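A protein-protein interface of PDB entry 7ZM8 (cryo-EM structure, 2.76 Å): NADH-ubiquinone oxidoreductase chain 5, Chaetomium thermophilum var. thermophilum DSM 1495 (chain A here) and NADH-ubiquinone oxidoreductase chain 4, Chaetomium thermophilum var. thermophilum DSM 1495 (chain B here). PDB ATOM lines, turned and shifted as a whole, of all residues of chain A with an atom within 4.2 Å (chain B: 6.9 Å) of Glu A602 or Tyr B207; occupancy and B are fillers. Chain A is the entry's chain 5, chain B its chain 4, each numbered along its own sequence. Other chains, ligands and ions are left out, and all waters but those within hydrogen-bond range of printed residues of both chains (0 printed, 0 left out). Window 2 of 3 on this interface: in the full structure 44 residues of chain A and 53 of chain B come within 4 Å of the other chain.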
ATOM      1  N   ASP A 597      -6.376   5.299  22.425  1.00  0.00           N
ATOM      2  CA  ASP A 597      -7.357   5.598  21.345  1.00  0.00           C
ATOM      3  C   ASP A 597      -7.953   6.985  21.509  1.00  0.00           C
ATOM      4  O   ASP A 597      -8.057   7.700  20.505  1.00  0.00           O
ATOM      5  CB  ASP A 597      -8.577   4.692  21.453  1.00  0.00           C
ATOM      6  CG  ASP A 597      -8.362   3.285  20.939  1.00  0.00           C
ATOM      7  OD1 ASP A 597      -7.700   3.140  19.898  1.00  0.00           O
ATOM      8  OD2 ASP A 597      -8.870   2.351  21.578  1.00  0.00           O
ATOM      9  N   GLY A 599      -6.674   9.076  23.650  1.00  0.00           N
ATOM     10  CA  GLY A 599      -5.621   9.882  24.219  1.00  0.00           C
ATOM     11  C   GLY A 599      -4.561  10.322  23.237  1.00  0.00           C
ATOM     12  O   GLY A 599      -4.741  11.282  22.485  1.00  0.00           O
ATOM     13  N   SER A 600      -3.439   9.606  23.254  1.00  0.00           N
ATOM     14  CA  SER A 600      -2.260  10.019  22.508  1.00  0.00           C
ATOM     15  C   SER A 600      -2.415   9.810  21.009  1.00  0.00           C
ATOM     16  O   SER A 600      -1.747  10.484  20.222  1.00  0.00           O
ATOM     17  CB  SER A 600      -1.046   9.264  23.033  1.00  0.00           C
ATOM     18  OG  SER A 600      -1.364   7.905  23.253  1.00  0.00           O
ATOM     19  N   ILE A 601      -3.352   8.970  20.609  1.00  0.00           N
ATOM     20  CA  ILE A 601      -3.465   8.690  19.161  1.00  0.00           C
ATOM     21  C   ILE A 601      -4.177   9.902  18.553  1.00  0.00           C
ATOM     22  O   ILE A 601      -3.880  10.253  17.402  1.00  0.00           O
ATOM     23  CB  ILE A 601      -4.169   7.339  18.911  1.00  0.00           C
ATOM     24  CG1 ILE A 601      -3.296   6.153  19.328  1.00  0.00           C
ATOM     25  CG2 ILE A 601      -4.641   7.204  17.474  1.00  0.00           C
ATOM     26  CD1 ILE A 601      -1.914   6.168  18.734  1.00  0.00           C
ATOM     27  N   GLU A 602      -5.047  10.552  19.332  1.00  0.00           N
ATOM     28  CA  GLU A 602      -5.695  11.749  18.816  1.00  0.00           C
ATOM     29  C   GLU A 602      -4.859  12.996  19.072  1.00  0.00           C
ATOM     30  O   GLU A 602      -4.899  13.942  18.281  1.00  0.00           O
ATOM     31  CB  GLU A 602      -7.093  11.901  19.410  1.00  0.00           C
ATOM     32  CG  GLU A 602      -7.998  10.728  19.128  1.00  0.00           C
ATOM     33  CD  GLU A 602      -9.455  11.124  19.065  1.00  0.00           C
ATOM     34  OE1 GLU A 602      -9.730  12.314  18.804  1.00  0.00           O
ATOM     35  OE2 GLU A 602     -10.327  10.254  19.278  1.00  0.00           O
ATOM     36  N   LEU A 603      -4.043  12.991  20.125  1.00  0.00           N
ATOM     37  CA  LEU A 603      -3.111  14.120  20.403  1.00  0.00           C
ATOM     38  C   LEU A 603      -1.949  14.088  19.410  1.00  0.00           C
ATOM     39  O   LEU A 603      -1.672  15.132  18.803  1.00  0.00           O
ATOM     40  CB  LEU A 603      -2.604  14.138  21.841  1.00  0.00           C
ATOM     41  CG  LEU A 603      -1.972  15.470  22.248  1.00  0.00           C
ATOM     42  CD1 LEU A 603      -2.843  16.641  21.820  1.00  0.00           C
ATOM     43  CD2 LEU A 603      -1.709  15.534  23.741  1.00  0.00           C
ATOM     44  N   PHE A 604      -1.270  12.952  19.265  1.00  0.00           N
ATOM     45  CA  PHE A 604      -0.240  12.874  18.198  1.00  0.00           C
ATOM     46  C   PHE A 604      -0.968  12.430  16.940  1.00  0.00           C
ATOM     47  O   PHE A 604      -0.645  11.368  16.393  1.00  0.00           O
ATOM     48  CB  PHE A 604       0.922  11.949  18.572  1.00  0.00           C
ATOM     49  CG  PHE A 604       2.126  12.010  17.669  1.00  0.00           C
ATOM     50  CD1 PHE A 604       2.904  13.150  17.601  1.00  0.00           C
ATOM     51  CD2 PHE A 604       2.497  10.912  16.912  1.00  0.00           C
ATOM     52  CE1 PHE A 604       4.017  13.200  16.778  1.00  0.00           C
ATOM     53  CE2 PHE A 604       3.609  10.962  16.088  1.00  0.00           C
ATOM     54  CZ  PHE A 604       4.368  12.106  16.024  1.00  0.00           C
ATOM     55  N   GLY A 605      -1.992  13.185  16.562  1.00  0.00           N
ATOM     56  CA  GLY A 605      -2.701  12.871  15.319  1.00  0.00           C
ATOM     57  C   GLY A 605      -3.685  13.941  14.925  1.00  0.00           C
ATOM     58  O   GLY A 605      -3.328  15.091  15.083  1.00  0.00           O
ATOM     59  N   PRO A 606      -4.953  13.622  14.551  1.00  0.00           N
ATOM     60  CA  PRO A 606      -5.870  14.632  13.996  1.00  0.00           C
ATOM     61  C   PRO A 606      -6.168  15.784  14.937  1.00  0.00           C
ATOM     62  O   PRO A 606      -6.212  16.936  14.499  1.00  0.00           O
ATOM     63  CB  PRO A 606      -7.137  13.820  13.695  1.00  0.00           C
ATOM     64  CG  PRO A 606      -6.730  12.406  13.748  1.00  0.00           C
ATOM     65  CD  PRO A 606      -5.606  12.315  14.706  1.00  0.00           C
ATOM     66  N   TYR A 607      -6.361  15.511  16.226  1.00  0.00           N
ATOM     67  CA  TYR A 607      -6.747  16.572  17.146  1.00  0.00           C
ATOM     68  C   TYR A 607      -5.573  17.489  17.462  1.00  0.00           C
ATOM     69  O   TYR A 607      -5.742  18.708  17.562  1.00  0.00           O
ATOM     70  CB  TYR A 607      -7.330  15.969  18.419  1.00  0.00           C
ATOM     71  CG  TYR A 607      -7.788  16.993  19.421  1.00  0.00           C
ATOM     72  CD1 TYR A 607      -8.805  17.882  19.118  1.00  0.00           C
ATOM     73  CD2 TYR A 607      -7.200  17.073  20.666  1.00  0.00           C
ATOM     74  CE1 TYR A 607      -9.223  18.813  20.034  1.00  0.00           C
ATOM     75  CE2 TYR A 607      -7.609  17.997  21.581  1.00  0.00           C
ATOM     76  CZ  TYR A 607      -8.619  18.865  21.266  1.00  0.00           C
ATOM     77  OH  TYR A 607      -9.022  19.797  22.193  1.00  0.00           O
ATOM     78  N   GLY A 608      -4.366  16.954  17.521  1.00  0.00           N
ATOM     79  CA  GLY A 608      -3.171  17.769  17.784  1.00  0.00           C
ATOM     80  C   GLY A 608      -2.716  18.518  16.553  1.00  0.00           C
ATOM     81  O   GLY A 608      -2.100  19.573  16.706  1.00  0.00           O
ATOM     82  N   PHE B 190     -18.996  11.954   2.184  1.00  0.00           N
ATOM     83  CA  PHE B 190     -18.923  13.143   3.023  1.00  0.00           C
ATOM     84  C   PHE B 190     -20.307  13.745   3.224  1.00  0.00           C
ATOM     85  O   PHE B 190     -20.657  14.170   4.330  1.00  0.00           O
ATOM     86  CB  PHE B 190     -17.963  14.155   2.395  1.00  0.00           C
ATOM     87  CG  PHE B 190     -17.811  15.423   3.173  1.00  0.00           C
ATOM     88  CD1 PHE B 190     -17.099  15.445   4.355  1.00  0.00           C
ATOM     89  CD2 PHE B 190     -18.373  16.601   2.716  1.00  0.00           C
ATOM     90  CE1 PHE B 190     -16.959  16.606   5.068  1.00  0.00           C
ATOM     91  CE2 PHE B 190     -18.236  17.770   3.432  1.00  0.00           C
ATOM     92  CZ  PHE B 190     -17.525  17.770   4.606  1.00  0.00           C
ATOM     93  N   LYS B 201     -21.843  14.058  13.614  1.00  0.00           N
ATOM     94  CA  LYS B 201     -21.687  13.833  12.155  1.00  0.00           C
ATOM     95  C   LYS B 201     -20.626  14.723  11.501  1.00  0.00           C
ATOM     96  O   LYS B 201     -19.945  14.221  10.612  1.00  0.00           O
ATOM     97  CB  LYS B 201     -23.048  14.039  11.477  1.00  0.00           C
ATOM     98  CG  LYS B 201     -23.667  15.423  11.593  1.00  0.00           C
ATOM     99  CD  LYS B 201     -24.981  15.516  10.868  1.00  0.00           C
ATOM    100  CE  LYS B 201     -25.537  16.921  10.838  1.00  0.00           C
ATOM    101  NZ  LYS B 201     -26.731  17.014   9.965  1.00  0.00           N
ATOM    102  N   VAL B 202     -20.529  15.996  11.888  1.00  0.00           N
ATOM    103  CA  VAL B 202     -19.613  16.912  11.157  1.00  0.00           C
ATOM    104  C   VAL B 202     -18.183  16.433  11.339  1.00  0.00           C
ATOM    105  O   VAL B 202     -17.488  16.306  10.334  1.00  0.00           O
ATOM    106  CB  VAL B 202     -19.802  18.401  11.498  1.00  0.00           C
ATOM    107  CG1 VAL B 202     -18.784  19.273  10.788  1.00  0.00           C
ATOM    108  CG2 VAL B 202     -21.206  18.867  11.158  1.00  0.00           C
ATOM    109  N   ARG B 203     -17.792  16.116  12.560  1.00  0.00           N
ATOM    110  CA  ARG B 203     -16.440  15.628  12.793  1.00  0.00           C
ATOM    111  C   ARG B 203     -16.244  14.247  12.184  1.00  0.00           C
ATOM    112  O   ARG B 203     -15.168  13.942  11.664  1.00  0.00           O
ATOM    113  CB  ARG B 203     -16.133  15.609  14.289  1.00  0.00           C
ATOM    114  CG  ARG B 203     -14.669  15.826  14.579  1.00  0.00           C
ATOM    115  CD  ARG B 203     -14.375  15.978  16.047  1.00  0.00           C
ATOM    116  NE  ARG B 203     -12.942  15.857  16.286  1.00  0.00           N
ATOM    117  CZ  ARG B 203     -12.098  16.878  16.297  1.00  0.00           C
ATOM    118  NH1 ARG B 203     -10.811  16.667  16.513  1.00  0.00           N
ATOM    119  NH2 ARG B 203     -12.540  18.109  16.094  1.00  0.00           N
ATOM    120  N   ALA B 204     -17.273  13.404  12.233  1.00  0.00           N
ATOM    121  CA  ALA B 204     -17.164  12.070  11.658  1.00  0.00           C
ATOM    122  C   ALA B 204     -16.918  12.135  10.157  1.00  0.00           C
ATOM    123  O   ALA B 204     -16.130  11.354   9.615  1.00  0.00           O
ATOM    124  CB  ALA B 204     -18.424  11.263  11.967  1.00  0.00           C
ATOM    125  N   SER B 205     -17.584  13.064   9.468  1.00  0.00           N
ATOM    126  CA  SER B 205     -17.426  13.166   8.023  1.00  0.00           C
ATOM    127  C   SER B 205     -16.103  13.817   7.643  1.00  0.00           C
ATOM    128  O   SER B 205     -15.537  13.493   6.594  1.00  0.00           O
ATOM    129  CB  SER B 205     -18.596  13.933   7.418  1.00  0.00           C
ATOM    130  OG  SER B 205     -18.627  15.263   7.888  1.00  0.00           O
ATOM    131  N   PHE B 206     -15.596  14.730   8.467  1.00  0.00           N
ATOM    132  CA  PHE B 206     -14.272  15.282   8.212  1.00  0.00           C
ATOM    133  C   PHE B 206     -13.190  14.228   8.402  1.00  0.00           C
ATOM    134  O   PHE B 206     -12.207  14.202   7.657  1.00  0.00           O
ATOM    135  CB  PHE B 206     -14.018  16.487   9.118  1.00  0.00           C
ATOM    136  CG  PHE B 206     -14.455  17.792   8.521  1.00  0.00           C
ATOM    137  CD1 PHE B 206     -15.774  18.194   8.590  1.00  0.00           C
ATOM    138  CD2 PHE B 206     -13.547  18.613   7.883  1.00  0.00           C
ATOM    139  CE1 PHE B 206     -16.177  19.386   8.039  1.00  0.00           C
ATOM    140  CE2 PHE B 206     -13.951  19.808   7.330  1.00  0.00           C
ATOM    141  CZ  PHE B 206     -15.267  20.189   7.407  1.00  0.00           C
ATOM    142  N   TYR B 207     -13.349  13.352   9.396  1.00  0.00           N
ATOM    143  CA  TYR B 207     -12.352  12.314   9.627  1.00  0.00           C
ATOM    144  C   TYR B 207     -12.249  11.356   8.452  1.00  0.00           C
ATOM    145  O   TYR B 207     -11.149  11.077   7.971  1.00  0.00           O
ATOM    146  CB  TYR B 207     -12.656  11.546  10.913  1.00  0.00           C
ATOM    147  CG  TYR B 207     -12.030  12.137  12.144  1.00  0.00           C
ATOM    148  CD1 TYR B 207     -12.252  13.453  12.500  1.00  0.00           C
ATOM    149  CD2 TYR B 207     -11.184  11.381  12.936  1.00  0.00           C
ATOM    150  CE1 TYR B 207     -11.670  13.992  13.620  1.00  0.00           C
ATOM    151  CE2 TYR B 207     -10.599  11.913  14.063  1.00  0.00           C
ATOM    152  CZ  TYR B 207     -10.847  13.220  14.399  1.00  0.00           C
ATOM    153  OH  TYR B 207     -10.265  13.757  15.520  1.00  0.00           O
ATOM    154  N   ILE B 208     -13.387  10.821   8.012  1.00  0.00           N
ATOM    155  CA  ILE B 208     -13.349   9.822   6.907  1.00  0.00           C
ATOM    156  C   ILE B 208     -12.738  10.474   5.664  1.00  0.00           C
ATOM    157  O   ILE B 208     -11.830   9.875   5.087  1.00  0.00           O
ATOM    158  CB  ILE B 208     -14.725   9.177   6.638  1.00  0.00           C
ATOM    159  CG1 ILE B 208     -14.646   8.114   5.540  1.00  0.00           C
ATOM    160  CG2 ILE B 208     -15.797  10.212   6.343  1.00  0.00           C
ATOM    161  CD1 ILE B 208     -15.991   7.651   5.039  1.00  0.00           C
ATOM    162  N   PHE B 209     -13.178  11.678   5.303  1.00  0.00           N
ATOM    163  CA  PHE B 209     -12.695  12.257   4.037  1.00  0.00           C
ATOM    164  C   PHE B 209     -11.195  12.517   4.143  1.00  0.00           C
ATOM    165  O   PHE B 209     -10.476  12.039   3.274  1.00  0.00           O
ATOM    166  CB  PHE B 209     -13.440  13.554   3.690  1.00  0.00           C
ATOM    167  CG  PHE B 209     -13.193  14.096   2.302  1.00  0.00           C
ATOM    168  CD1 PHE B 209     -12.007  14.737   1.979  1.00  0.00           C
ATOM    169  CD2 PHE B 209     -14.160  13.982   1.319  1.00  0.00           C
ATOM    170  CE1 PHE B 209     -11.786  15.235   0.706  1.00  0.00           C
ATOM    171  CE2 PHE B 209     -13.941  14.482   0.047  1.00  0.00           C
ATOM    172  CZ  PHE B 209     -12.754  15.103  -0.259  1.00  0.00           C
ATOM    173  N   LEU B 210     -10.748  13.244   5.167  1.00  0.00           N
ATOM    174  CA  LEU B 210      -9.325  13.674   5.253  1.00  0.00           C
ATOM    175  C   LEU B 210      -8.355  12.507   5.434  1.00  0.00           C
ATOM    176  O   LEU B 210      -7.291  12.560   4.812  1.00  0.00           O
ATOM    177  CB  LEU B 210      -9.184  14.734   6.348  1.00  0.00           C
ATOM    178  CG  LEU B 210      -9.885  16.057   6.053  1.00  0.00           C
ATOM    179  CD1 LEU B 210      -9.910  16.946   7.284  1.00  0.00           C
ATOM    180  CD2 LEU B 210      -9.230  16.771   4.882  1.00  0.00           C
ATOM    181  N   TYR B 211      -8.677  11.520   6.267  1.00  0.00           N
ATOM    182  CA  TYR B 211      -7.810  10.322   6.416  1.00  0.00           C
ATOM    183  C   TYR B 211      -7.760   9.545   5.104  1.00  0.00           C
ATOM    184  O   TYR B 211      -6.675   9.094   4.719  1.00  0.00           O
ATOM    185  CB  TYR B 211      -8.398   9.373   7.457  1.00  0.00           C
ATOM    186  CG  TYR B 211      -7.645   9.264   8.757  1.00  0.00           C
ATOM    187  CD1 TYR B 211      -6.501   8.492   8.856  1.00  0.00           C
ATOM    188  CD2 TYR B 211      -8.098   9.904   9.896  1.00  0.00           C
ATOM    189  CE1 TYR B 211      -5.812   8.375  10.051  1.00  0.00           C
ATOM    190  CE2 TYR B 211      -7.418   9.802  11.097  1.00  0.00           C
ATOM    191  CZ  TYR B 211      -6.273   9.032  11.175  1.00  0.00           C
ATOM    192  OH  TYR B 211      -5.600   8.923  12.356  1.00  0.00           O
ATOM    193  N   THR B 212      -8.909   9.370   4.457  1.00  0.00           N
ATOM    194  CA  THR B 212      -8.964   8.570   3.209  1.00  0.00           C
ATOM    195  C   THR B 212      -8.308   9.371   2.093  1.00  0.00           C
ATOM    196  O   THR B 212      -7.699   8.753   1.217  1.00  0.00           O
ATOM    197  CB  THR B 212     -10.402   8.153   2.879  1.00  0.00           C
ATOM    198  OG1 THR B 212     -10.935   7.469   4.013  1.00  0.00           O
ATOM    199  CG2 THR B 212     -10.511   7.272   1.655  1.00  0.00           C
ATOM    200  N   LEU B 213      -8.427  10.697   2.138  1.00  0.00           N
ATOM    201  CA  LEU B 213      -7.724  11.484   1.136  1.00  0.00           C
ATOM    202  C   LEU B 213      -6.222  11.450   1.359  1.00  0.00           C
ATOM    203  O   LEU B 213      -5.455  11.295   0.406  1.00  0.00           O
ATOM    204  CB  LEU B 213      -8.225  12.930   1.154  1.00  0.00           C
ATOM    205  CG  LEU B 213      -7.536  13.884   0.180  1.00  0.00           C
ATOM    206  CD1 LEU B 213      -8.000  13.622  -1.228  1.00  0.00           C
ATOM    207  CD2 LEU B 213      -7.755  15.323   0.582  1.00  0.00           C
ATOM    208  N   SER B 270      -9.238   5.754  13.818  1.00  0.00           N
ATOM    209  CA  SER B 270     -10.118   6.772  14.461  1.00  0.00           C
ATOM    210  C   SER B 270     -11.268   7.200  13.556  1.00  0.00           C
ATOM    211  O   SER B 270     -12.360   7.472  14.075  1.00  0.00           O
ATOM    212  CB  SER B 270      -9.304   7.963  14.840  1.00  0.00           C
ATOM    213  OG  SER B 270      -8.483   8.374  13.760  1.00  0.00           O
ATOM    214  N   TRP B 271     -11.007   7.296  12.254  1.00  0.00           N
ATOM    215  CA  TRP B 271     -12.030   7.716  11.266  1.00  0.00           C
ATOM    216  C   TRP B 271     -13.203   6.741  11.269  1.00  0.00           C
ATOM    217  O   TRP B 271     -14.321   7.217  11.162  1.00  0.00           O
ATOM    218  CB  TRP B 271     -11.389   7.848   9.882  1.00  0.00           C
ATOM    219  CG  TRP B 271     -10.772   6.592   9.351  1.00  0.00           C
ATOM    220  CD1 TRP B 271      -9.488   6.169   9.528  1.00  0.00           C
ATOM    221  CD2 TRP B 271     -11.415   5.597   8.536  1.00  0.00           C
ATOM    222  NE1 TRP B 271      -9.292   4.974   8.894  1.00  0.00           N
ATOM    223  CE2 TRP B 271     -10.455   4.599   8.277  1.00  0.00           C
ATOM    224  CE3 TRP B 271     -12.703   5.449   8.012  1.00  0.00           C
ATOM    225  CZ2 TRP B 271     -10.746   3.471   7.513  1.00  0.00           C
ATOM    226  CZ3 TRP B 271     -12.991   4.332   7.263  1.00  0.00           C
ATOM    227  CH2 TRP B 271     -12.023   3.359   7.018  1.00  0.00           C
ATOM    228  N   LEU B 272     -12.954   5.440  11.370  1.00  0.00           N
ATOM    229  CA  LEU B 272     -14.013   4.406  11.315  1.00  0.00           C
ATOM    230  C   LEU B 272     -14.853   4.470  12.590  1.00  0.00           C
ATOM    231  O   LEU B 272     -16.072   4.340  12.509  1.00  0.00           O
ATOM    232  CB  LEU B 272     -13.256   3.085  11.147  1.00  0.00           C
ATOM    233  CG  LEU B 272     -14.079   1.831  10.893  1.00  0.00           C
ATOM    234  CD1 LEU B 272     -13.474   1.052   9.745  1.00  0.00           C
ATOM    235  CD2 LEU B 272     -14.144   0.972  12.137  1.00  0.00           C
ATOM    236  N   ARG B 274     -15.526   6.962  14.219  1.00  0.00           N
ATOM    237  CA  ARG B 274     -16.439   8.106  14.019  1.00  0.00           C
ATOM    238  C   ARG B 274     -17.354   7.840  12.815  1.00  0.00           C
ATOM    239  O   ARG B 274     -18.548   7.821  13.044  1.00  0.00           O
ATOM    240  CB  ARG B 274     -15.574   9.362  13.889  1.00  0.00           C
ATOM    241  CG  ARG B 274     -14.842   9.761  15.158  1.00  0.00           C
ATOM    242  CD  ARG B 274     -14.310  11.175  15.063  1.00  0.00           C
ATOM    243  NE  ARG B 274     -13.431  11.465  16.186  1.00  0.00           N
ATOM    244  CZ  ARG B 274     -13.786  12.115  17.287  1.00  0.00           C
ATOM    245  NH1 ARG B 274     -12.900  12.316  18.244  1.00  0.00           N
ATOM    246  NH2 ARG B 274     -15.019  12.567  17.424  1.00  0.00           N
ATOM    247  N   ALA B 275     -16.828   7.622  11.605  1.00  0.00           N
ATOM    248  CA  ALA B 275     -17.617   7.440  10.362  1.00  0.00           C
ATOM    249  C   ALA B 275     -18.768   6.447  10.522  1.00  0.00           C
ATOM    250  O   ALA B 275     -19.901   6.854  10.278  1.00  0.00           O
ATOM    251  CB  ALA B 275     -16.709   7.007   9.238  1.00  0.00           C
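The guanidinium group of Arg B274 lies within salt-bridge range of the side-chain carboxylate of Glu A602 (3.2 Å).
Among the printed residues, merely in contact across the chains: Tyr A607 with Arg B203 (3.5 Å), Pro A606 with Tyr B207 (3.6 Å), Glu A602 with Tyr B207 (3.6 Å) and Pro A606 with Tyr B211 (3.8 Å).
OH of Tyr B207 lies within hydrogen-bond range of NH1 of Arg B203 (3.1 Å).
The side-chain hydroxyl (OG) of Ser B270 lies close to the side-chain hydroxyl (OH) of Tyr B211 (3.3 Å).
The backbone NH (N) of Tyr A607 is in hydrogen-bond range of the backbone carbonyl oxygen (O) of Glu A602 (3.0 Å).
The backbone NH (N) of Gly A608 lies within hydrogen-bond range of the backbone carbonyl oxygen (O) of Glu A602, 3.2 Å away.
Glu A602 touches just these residues of chain B: Tyr B207 and Arg B274.
Printed residues of chain B within 4 Å of Pro A606: Tyr B207 (3.6 Å) and Tyr B211 (3.8 Å).
Of chain A, only Glu A602 and Pro A606 come within 4 Å of Tyr B207.
Printed residues of chain A within 4 Å of Arg B274: Glu A602.
The nearest residue of chain B that does not touch Glu A602 is Arg B203 (5.0 Å).
Of the 11 printed residues of chain A, 3 touch a printed residue of chain B.
Hydrophobic or aromatic side chains of chain A that line the printed part of chain B: Pro A606 and Tyr A607.
Of the 19 printed residues of chain B, 4 touch a printed residue of chain A.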
